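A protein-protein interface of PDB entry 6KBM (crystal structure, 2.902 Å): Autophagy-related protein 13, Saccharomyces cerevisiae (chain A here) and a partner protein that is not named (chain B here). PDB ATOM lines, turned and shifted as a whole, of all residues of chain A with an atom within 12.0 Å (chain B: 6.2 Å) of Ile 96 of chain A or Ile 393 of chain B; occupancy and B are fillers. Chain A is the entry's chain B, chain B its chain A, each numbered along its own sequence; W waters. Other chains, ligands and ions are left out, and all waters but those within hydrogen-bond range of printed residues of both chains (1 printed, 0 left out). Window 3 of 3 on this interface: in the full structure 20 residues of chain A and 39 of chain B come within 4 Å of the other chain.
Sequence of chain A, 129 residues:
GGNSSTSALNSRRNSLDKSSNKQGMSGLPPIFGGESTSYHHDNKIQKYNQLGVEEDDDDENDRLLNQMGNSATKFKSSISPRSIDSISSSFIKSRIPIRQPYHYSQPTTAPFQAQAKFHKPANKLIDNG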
ATOM      1  N   SER A  94     -27.159  27.127  19.157  1.00  0.00           N
ATOM      2  CA  SER A  94     -27.254  26.806  17.739  1.00  0.00           C
ATOM      3  C   SER A  94     -26.217  25.752  17.344  1.00  0.00           C
ATOM      4  O   SER A  94     -26.274  25.188  16.254  1.00  0.00           O
ATOM      5  CB  SER A  94     -27.074  28.073  16.892  1.00  0.00           C
ATOM      6  OG  SER A  94     -26.511  27.769  15.628  1.00  0.00           O
ATOM      7  N   ARG A  95     -25.250  25.504  18.222  1.00  0.00           N
ATOM      8  CA  ARG A  95     -24.214  24.512  17.948  1.00  0.00           C
ATOM      9  C   ARG A  95     -24.450  23.246  18.772  1.00  0.00           C
ATOM     10  O   ARG A  95     -23.523  22.676  19.351  1.00  0.00           O
ATOM     11  CB  ARG A  95     -22.827  25.093  18.228  1.00  0.00           C
ATOM     12  CG  ARG A  95     -21.780  24.697  17.207  1.00  0.00           C
ATOM     13  CD  ARG A  95     -20.487  25.483  17.381  1.00  0.00           C
ATOM     14  NE  ARG A  95     -20.676  26.909  17.121  1.00  0.00           N
ATOM     15  CZ  ARG A  95     -20.411  27.500  15.961  1.00  0.00           C
ATOM     16  NH1 ARG A  95     -19.932  26.791  14.949  1.00  0.00           N
ATOM     17  NH2 ARG A  95     -20.617  28.802  15.814  1.00  0.00           N
ATOM     18  N   ILE A  96     -25.711  22.825  18.816  1.00  0.00           N
ATOM     19  CA  ILE A  96     -26.123  21.596  19.486  1.00  0.00           C
ATOM     20  C   ILE A  96     -25.442  20.387  18.840  1.00  0.00           C
ATOM     21  O   ILE A  96     -25.080  20.434  17.663  1.00  0.00           O
ATOM     22  CB  ILE A  96     -27.670  21.434  19.429  1.00  0.00           C
ATOM     23  CG1 ILE A  96     -28.226  20.910  20.756  1.00  0.00           C
ATOM     24  CG2 ILE A  96     -28.100  20.563  18.252  1.00  0.00           C
ATOM     25  CD1 ILE A  96     -28.172  21.916  21.881  1.00  0.00           C
ATOM     26  N   PRO A  97     -25.230  19.309  19.612  1.00  0.00           N
ATOM     27  CA  PRO A  97     -24.778  18.068  18.973  1.00  0.00           C
ATOM     28  C   PRO A  97     -25.882  17.463  18.109  1.00  0.00           C
ATOM     29  O   PRO A  97     -27.024  17.358  18.557  1.00  0.00           O
ATOM     30  CB  PRO A  97     -24.435  17.160  20.159  1.00  0.00           C
ATOM     31  CG  PRO A  97     -25.189  17.730  21.311  1.00  0.00           C
ATOM     32  CD  PRO A  97     -25.216  19.208  21.081  1.00  0.00           C
ATOM     33  N   ILE A  98     -25.544  17.074  16.884  1.00  0.00           N
ATOM     34  CA  ILE A  98     -26.548  16.610  15.932  1.00  0.00           C
ATOM     35  C   ILE A  98     -26.767  15.102  16.001  1.00  0.00           C
ATOM     36  O   ILE A  98     -25.815  14.323  16.066  1.00  0.00           O
ATOM     37  CB  ILE A  98     -26.168  16.984  14.489  1.00  0.00           C
ATOM     38  CG1 ILE A  98     -25.659  18.425  14.430  1.00  0.00           C
ATOM     39  CG2 ILE A  98     -27.356  16.792  13.558  1.00  0.00           C
ATOM     40  CD1 ILE A  98     -25.333  18.897  13.031  1.00  0.00           C
ATOM     41  N   ARG A  99     -28.036  14.705  15.988  1.00  0.00           N
ATOM     42  CA  ARG A  99     -28.407  13.297  15.978  1.00  0.00           C
ATOM     43  C   ARG A  99     -28.132  12.678  14.615  1.00  0.00           C
ATOM     44  O   ARG A  99     -28.553  13.211  13.587  1.00  0.00           O
ATOM     45  CB  ARG A  99     -29.885  13.131  16.337  1.00  0.00           C
ATOM     46  CG  ARG A  99     -30.342  11.687  16.445  1.00  0.00           C
ATOM     47  CD  ARG A  99     -31.856  11.603  16.546  1.00  0.00           C
ATOM     48  NE  ARG A  99     -32.513  12.300  15.443  1.00  0.00           N
ATOM     49  CZ  ARG A  99     -32.919  11.715  14.320  1.00  0.00           C
ATOM     50  NH1 ARG A  99     -32.740  10.412  14.141  1.00  0.00           N
ATOM     51  NH2 ARG A  99     -33.507  12.434  13.373  1.00  0.00           N
ATOM     52  N   GLN A 100     -27.418  11.556  14.615  1.00  0.00           N
ATOM     53  CA  GLN A 100     -27.165  10.812  13.390  1.00  0.00           C
ATOM     54  C   GLN A 100     -28.491  10.403  12.755  1.00  0.00           C
ATOM     55  O   GLN A 100     -29.433  10.048  13.462  1.00  0.00           O
ATOM     56  CB  GLN A 100     -26.304   9.578  13.674  1.00  0.00           C
ATOM     57  CG  GLN A 100     -25.085   9.844  14.549  1.00  0.00           C
ATOM     58  CD  GLN A 100     -24.031  10.695  13.861  1.00  0.00           C
ATOM     59  OE1 GLN A 100     -24.025  10.832  12.637  1.00  0.00           O
ATOM     60  NE2 GLN A 100     -23.129  11.268  14.650  1.00  0.00           N
ATOM     61  N   HIS A 103     -29.779   7.293  13.950  1.00  0.00           N
ATOM     62  CA  HIS A 103     -29.820   7.173  15.397  1.00  0.00           C
ATOM     63  C   HIS A 103     -31.257   7.271  15.893  1.00  0.00           C
ATOM     64  O   HIS A 103     -31.710   8.325  16.339  1.00  0.00           O
ATOM     65  CB  HIS A 103     -28.951   8.233  16.072  1.00  0.00           C
ATOM     66  CG  HIS A 103     -28.683   7.951  17.516  1.00  0.00           C
ATOM     67  ND1 HIS A 103     -28.116   6.772  17.948  1.00  0.00           N
ATOM     68  CD2 HIS A 103     -28.917   8.686  18.629  1.00  0.00           C
ATOM     69  CE1 HIS A 103     -28.005   6.795  19.264  1.00  0.00           C
ATOM     70  NE2 HIS A 103     -28.485   7.944  19.701  1.00  0.00           N
ATOM     71  N   LEU B 349     -34.641  11.302  26.345  1.00  0.00           N
ATOM     72  CA  LEU B 349     -34.308  12.503  27.105  1.00  0.00           C
ATOM     73  C   LEU B 349     -33.506  13.488  26.259  1.00  0.00           C
ATOM     74  O   LEU B 349     -33.772  14.695  26.267  1.00  0.00           O
ATOM     75  CB  LEU B 349     -33.529  12.135  28.371  1.00  0.00           C
ATOM     76  CG  LEU B 349     -34.289  11.316  29.417  1.00  0.00           C
ATOM     77  CD1 LEU B 349     -33.355  10.850  30.522  1.00  0.00           C
ATOM     78  CD2 LEU B 349     -35.448  12.117  29.993  1.00  0.00           C
ATOM     79  N   ARG B 350     -32.534  12.959  25.520  1.00  0.00           N
ATOM     80  CA  ARG B 350     -31.714  13.761  24.622  1.00  0.00           C
ATOM     81  C   ARG B 350     -32.573  14.470  23.589  1.00  0.00           C
ATOM     82  O   ARG B 350     -32.390  15.656  23.336  1.00  0.00           O
ATOM     83  CB  ARG B 350     -30.671  12.896  23.914  1.00  0.00           C
ATOM     84  CG  ARG B 350     -29.950  13.627  22.793  1.00  0.00           C
ATOM     85  CD  ARG B 350     -29.260  12.669  21.838  1.00  0.00           C
ATOM     86  NE  ARG B 350     -28.469  13.379  20.836  1.00  0.00           N
ATOM     87  CZ  ARG B 350     -27.541  12.807  20.076  1.00  0.00           C
ATOM     88  NH1 ARG B 350     -27.286  11.512  20.203  1.00  0.00           N
ATOM     89  NH2 ARG B 350     -26.869  13.529  19.190  1.00  0.00           N
ATOM     90  N   ASN B 351     -33.506  13.733  22.992  1.00  0.00           N
ATOM     91  CA  ASN B 351     -34.434  14.308  22.023  1.00  0.00           C
ATOM     92  C   ASN B 351     -35.231  15.459  22.629  1.00  0.00           C
ATOM     93  O   ASN B 351     -35.267  16.571  22.082  1.00  0.00           O
ATOM     94  CB  ASN B 351     -35.389  13.235  21.494  1.00  0.00           C
ATOM     95  CG  ASN B 351     -34.681  12.168  20.677  1.00  0.00           C
ATOM     96  OD1 ASN B 351     -33.460  12.187  20.529  1.00  0.00           O
ATOM     97  ND2 ASN B 351     -35.451  11.226  20.144  1.00  0.00           N
ATOM     98  N   ALA B 353     -34.681  17.288  25.261  1.00  0.00           N
ATOM     99  CA  ALA B 353     -33.846  18.439  25.593  1.00  0.00           C
ATOM    100  C   ALA B 353     -33.414  19.205  24.343  1.00  0.00           C
ATOM    101  O   ALA B 353     -33.415  20.436  24.326  1.00  0.00           O
ATOM    102  CB  ALA B 353     -32.628  17.991  26.385  1.00  0.00           C
ATOM    103  N   ALA B 354     -33.047  18.466  23.302  1.00  0.00           N
ATOM    104  CA  ALA B 354     -32.538  19.057  22.070  1.00  0.00           C
ATOM    105  C   ALA B 354     -33.606  19.848  21.327  1.00  0.00           C
ATOM    106  O   ALA B 354     -33.292  20.814  20.631  1.00  0.00           O
ATOM    107  CB  ALA B 354     -31.966  17.979  21.165  1.00  0.00           C
ATOM    108  N   SER B 355     -34.862  19.432  21.469  1.00  0.00           N
ATOM    109  CA  SER B 355     -35.959  20.090  20.763  1.00  0.00           C
ATOM    110  C   SER B 355     -36.232  21.567  21.056  1.00  0.00           C
ATOM    111  O   SER B 355     -36.225  22.389  20.141  1.00  0.00           O
ATOM    112  CB  SER B 355     -37.282  19.380  21.055  1.00  0.00           C
ATOM    113  OG  SER B 355     -37.222  18.021  20.654  1.00  0.00           O
ATOM    114  N   ARG B 360     -37.458  23.370  29.857  1.00  0.00           N
ATOM    115  CA  ARG B 360     -36.212  23.103  30.575  1.00  0.00           C
ATOM    116  C   ARG B 360     -36.376  22.951  32.077  1.00  0.00           C
ATOM    117  O   ARG B 360     -35.807  22.041  32.680  1.00  0.00           O
ATOM    118  CB  ARG B 360     -35.133  24.164  30.308  1.00  0.00           C
ATOM    119  CG  ARG B 360     -34.471  24.103  28.948  1.00  0.00           C
ATOM    120  CD  ARG B 360     -33.843  22.750  28.711  1.00  0.00           C
ATOM    121  NE  ARG B 360     -33.258  22.643  27.380  1.00  0.00           N
ATOM    122  CZ  ARG B 360     -32.003  22.966  27.092  1.00  0.00           C
ATOM    123  NH1 ARG B 360     -31.202  23.427  28.044  1.00  0.00           N
ATOM    124  NH2 ARG B 360     -31.551  22.834  25.854  1.00  0.00           N
ATOM    125  N   SER B 388     -23.641  11.855  27.322  1.00  0.00           N
ATOM    126  CA  SER B 388     -22.656  12.823  26.864  1.00  0.00           C
ATOM    127  C   SER B 388     -23.292  13.860  25.943  1.00  0.00           C
ATOM    128  O   SER B 388     -23.104  15.069  26.121  1.00  0.00           O
ATOM    129  CB  SER B 388     -21.514  12.100  26.152  1.00  0.00           C
ATOM    130  OG  SER B 388     -20.809  12.970  25.292  1.00  0.00           O
ATOM    131  N   ALA B 389     -24.048  13.377  24.961  1.00  0.00           N
ATOM    132  CA  ALA B 389     -24.767  14.258  24.048  1.00  0.00           C
ATOM    133  C   ALA B 389     -25.744  15.141  24.816  1.00  0.00           C
ATOM    134  O   ALA B 389     -25.865  16.337  24.546  1.00  0.00           O
ATOM    135  CB  ALA B 389     -25.502  13.446  22.990  1.00  0.00           C
ATOM    136  N   CYS B 390     -26.427  14.539  25.784  1.00  0.00           N
ATOM    137  CA  CYS B 390     -27.408  15.246  26.599  1.00  0.00           C
ATOM    138  C   CYS B 390     -26.771  16.406  27.366  1.00  0.00           C
ATOM    139  O   CYS B 390     -27.277  17.530  27.351  1.00  0.00           O
ATOM    140  CB  CYS B 390     -28.080  14.273  27.568  1.00  0.00           C
ATOM    141  SG  CYS B 390     -29.680  14.815  28.189  1.00  0.00           S
ATOM    142  N   PHE B 391     -25.653  16.126  28.030  1.00  0.00           N
ATOM    143  CA  PHE B 391     -24.886  17.151  28.732  1.00  0.00           C
ATOM    144  C   PHE B 391     -24.460  18.254  27.776  1.00  0.00           C
ATOM    145  O   PHE B 391     -24.613  19.439  28.076  1.00  0.00           O
ATOM    146  CB  PHE B 391     -23.650  16.545  29.401  1.00  0.00           C
ATOM    147  CG  PHE B 391     -23.950  15.777  30.653  1.00  0.00           C
ATOM    148  CD1 PHE B 391     -25.103  16.024  31.376  1.00  0.00           C
ATOM    149  CD2 PHE B 391     -23.070  14.811  31.111  1.00  0.00           C
ATOM    150  CE1 PHE B 391     -25.376  15.319  32.530  1.00  0.00           C
ATOM    151  CE2 PHE B 391     -23.337  14.103  32.266  1.00  0.00           C
ATOM    152  CZ  PHE B 391     -24.491  14.356  32.975  1.00  0.00           C
ATOM    153  N   ALA B 392     -23.922  17.851  26.627  1.00  0.00           N
ATOM    154  CA  ALA B 392     -23.505  18.797  25.598  1.00  0.00           C
ATOM    155  C   ALA B 392     -24.649  19.736  25.223  1.00  0.00           C
ATOM    156  O   ALA B 392     -24.437  20.928  24.995  1.00  0.00           O
ATOM    157  CB  ALA B 392     -23.003  18.056  24.372  1.00  0.00           C
ATOM    158  N   ILE B 393     -25.860  19.190  25.167  1.00  0.00           N
ATOM    159  CA  ILE B 393     -27.052  19.985  24.887  1.00  0.00           C
ATOM    160  C   ILE B 393     -27.356  20.967  26.014  1.00  0.00           C
ATOM    161  O   ILE B 393     -27.530  22.163  25.778  1.00  0.00           O
ATOM    162  CB  ILE B 393     -28.286  19.092  24.666  1.00  0.00           C
ATOM    163  CG1 ILE B 393     -28.117  18.251  23.402  1.00  0.00           C
ATOM    164  CG2 ILE B 393     -29.549  19.934  24.577  1.00  0.00           C
ATOM    165  CD1 ILE B 393     -29.132  17.146  23.275  1.00  0.00           C
ATOM    166  N   LEU B 394     -27.422  20.452  27.238  1.00  0.00           N
ATOM    167  CA  LEU B 394     -27.798  21.262  28.393  1.00  0.00           C
ATOM    168  C   LEU B 394     -26.827  22.406  28.668  1.00  0.00           C
ATOM    169  O   LEU B 394     -27.233  23.476  29.122  1.00  0.00           O
ATOM    170  CB  LEU B 394     -27.912  20.383  29.637  1.00  0.00           C
ATOM    171  CG  LEU B 394     -29.111  19.440  29.685  1.00  0.00           C
ATOM    172  CD1 LEU B 394     -29.128  18.675  30.999  1.00  0.00           C
ATOM    173  CD2 LEU B 394     -30.405  20.215  29.494  1.00  0.00           C
ATOM    174  N   ALA B 395     -25.547  22.184  28.386  1.00  0.00           N
ATOM    175  CA  ALA B 395     -24.517  23.173  28.691  1.00  0.00           C
ATOM    176  C   ALA B 395     -24.477  24.313  27.676  1.00  0.00           C
ATOM    177  O   ALA B 395     -23.542  25.114  27.670  1.00  0.00           O
ATOM    178  CB  ALA B 395     -23.158  22.501  28.774  1.00  0.00           C
ATOM    179  N   LEU B 396     -25.490  24.387  26.819  1.00  0.00           N
ATOM    180  CA  LEU B 396     -25.573  25.450  25.824  1.00  0.00           C
ATOM    181  C   LEU B 396     -26.626  26.489  26.198  1.00  0.00           C
ATOM    182  O   LEU B 396     -26.769  27.513  25.529  1.00  0.00           O
ATOM    183  CB  LEU B 396     -25.870  24.868  24.441  1.00  0.00           C
ATOM    184  CG  LEU B 396     -24.666  24.217  23.759  1.00  0.00           C
ATOM    185  CD1 LEU B 396     -25.045  23.630  22.414  1.00  0.00           C
ATOM    186  CD2 LEU B 396     -23.558  25.237  23.602  1.00  0.00           C
ATOM    187  N   ALA B 397     -27.364  26.215  27.268  1.00  0.00           N
ATOM    188  CA  ALA B 397     -28.321  27.176  27.799  1.00  0.00           C
ATOM    189  C   ALA B 397     -27.618  28.100  28.788  1.00  0.00           C
ATOM    190  O   ALA B 397     -27.246  27.679  29.884  1.00  0.00           O
ATOM    191  CB  ALA B 397     -29.486  26.463  28.462  1.00  0.00           C
ATOM    192  N   ALA B 431     -19.032  20.495  26.303  1.00  0.00           N
ATOM    193  CA  ALA B 431     -19.895  20.960  27.384  1.00  0.00           C
ATOM    194  C   ALA B 431     -19.081  21.703  28.435  1.00  0.00           C
ATOM    195  O   ALA B 431     -19.436  22.813  28.849  1.00  0.00           O
ATOM    196  CB  ALA B 431     -20.639  19.791  28.013  1.00  0.00           C
HETATM  197  O   HOH W   1     -28.952  15.491  19.663  1.00  0.00           O
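NH2 of Arg 350 of chain B is in hydrogen-bond range of O of Ile 98 of chain A.
The guanidinium group of Arg 99 of chain A sits at hydrogen-bond distance from the backbone carbonyl oxygen of His 103 of chain A.
O of Arg 95 of chain A touches CD1 of Leu 396 of chain B, at 3.6 Å. Ile 393 of chain B touches Ile 96 of chain A. Leu 396 of chain B touches Ile 96 of chain A (CD1 to CD1, 3.6 Å). O of Pro 97 of chain A touches NH2 of Arg 350 of chain B, at 3.9 Å. Ala 389 of chain B touches Pro 97 of chain A (O to CG, 3.6 Å). Ala 392 of chain B touches Pro 97 of chain A. CG1 of Ile 393 of chain B touches CG of Pro 97 of chain A (3.6 Å). Arg 350 of chain B touches Arg 99 of chain A. His 103 of chain A touches Arg 350 of chain B (CD2 to NH1, 3.6 Å).
Printed residues of chain B within 4 Å of Ile 96 of chain A: Ile 393 and Leu 396. Ile 393 of chain B touches two residues of chain A. Arg 350 of chain B touches just these residues of chain A: Pro 97 (3.9 Å), Ile 98 (3.4 Å), Arg 99 (3.6 Å) and His 103 (3.6 Å). No residue of chain A comes within 4 Å of Ala 354 of chain B. Ala 389 of chain B touches just one residue of chain A: Pro 97. No residue of chain A comes within 4 Å of Cys 390 of chain B. Printed residues of chain A within 4 Å of Ala 392 of chain B: Pro 97 (3.8 Å). Leu 394 of chain B touches none of the printed residues of chain A. No residue of chain A comes within 4 Å of Ala 395 of chain B. Leu 396 of chain B touches just these residues of chain A: Arg 95 (3.6 Å) and Ile 96 (3.6 Å). No residue of chain A comes within 4 Å of Ala 397 of chain B. Printed residues of chain B within 4 Å of Ile 98 of chain A: Arg 350. Printed residues of chain B within 4 Å of His 103 of chain A: Arg 350 (3.6 Å). Of the printed residues of chain B, Arg 99 of chain A touches Arg 350 (3.6 Å). Phe 391 of chain B touches none of the printed residues of chain A. Ala 431 of chain B touches none of the printed residues of chain A. The nearest printed residue of chain A that does not touch Ile 393 of chain B is Arg 95 of chain A (7.1 Å).
Of the 18 printed residues of chain B, 5 touch a printed residue of chain A. Among the printed residues, 10 pairs touch across the chains. Among the printed residues, no Asp or Glu carboxylate lies within 4 Å of a Lys or Arg side-chain nitrogen of the other chain.
Water W1 lies within hydrogen-bond range of NE of Arg 350 of chain B (2.5 Å) and O of Pro 97 of chain A (2.9 Å).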
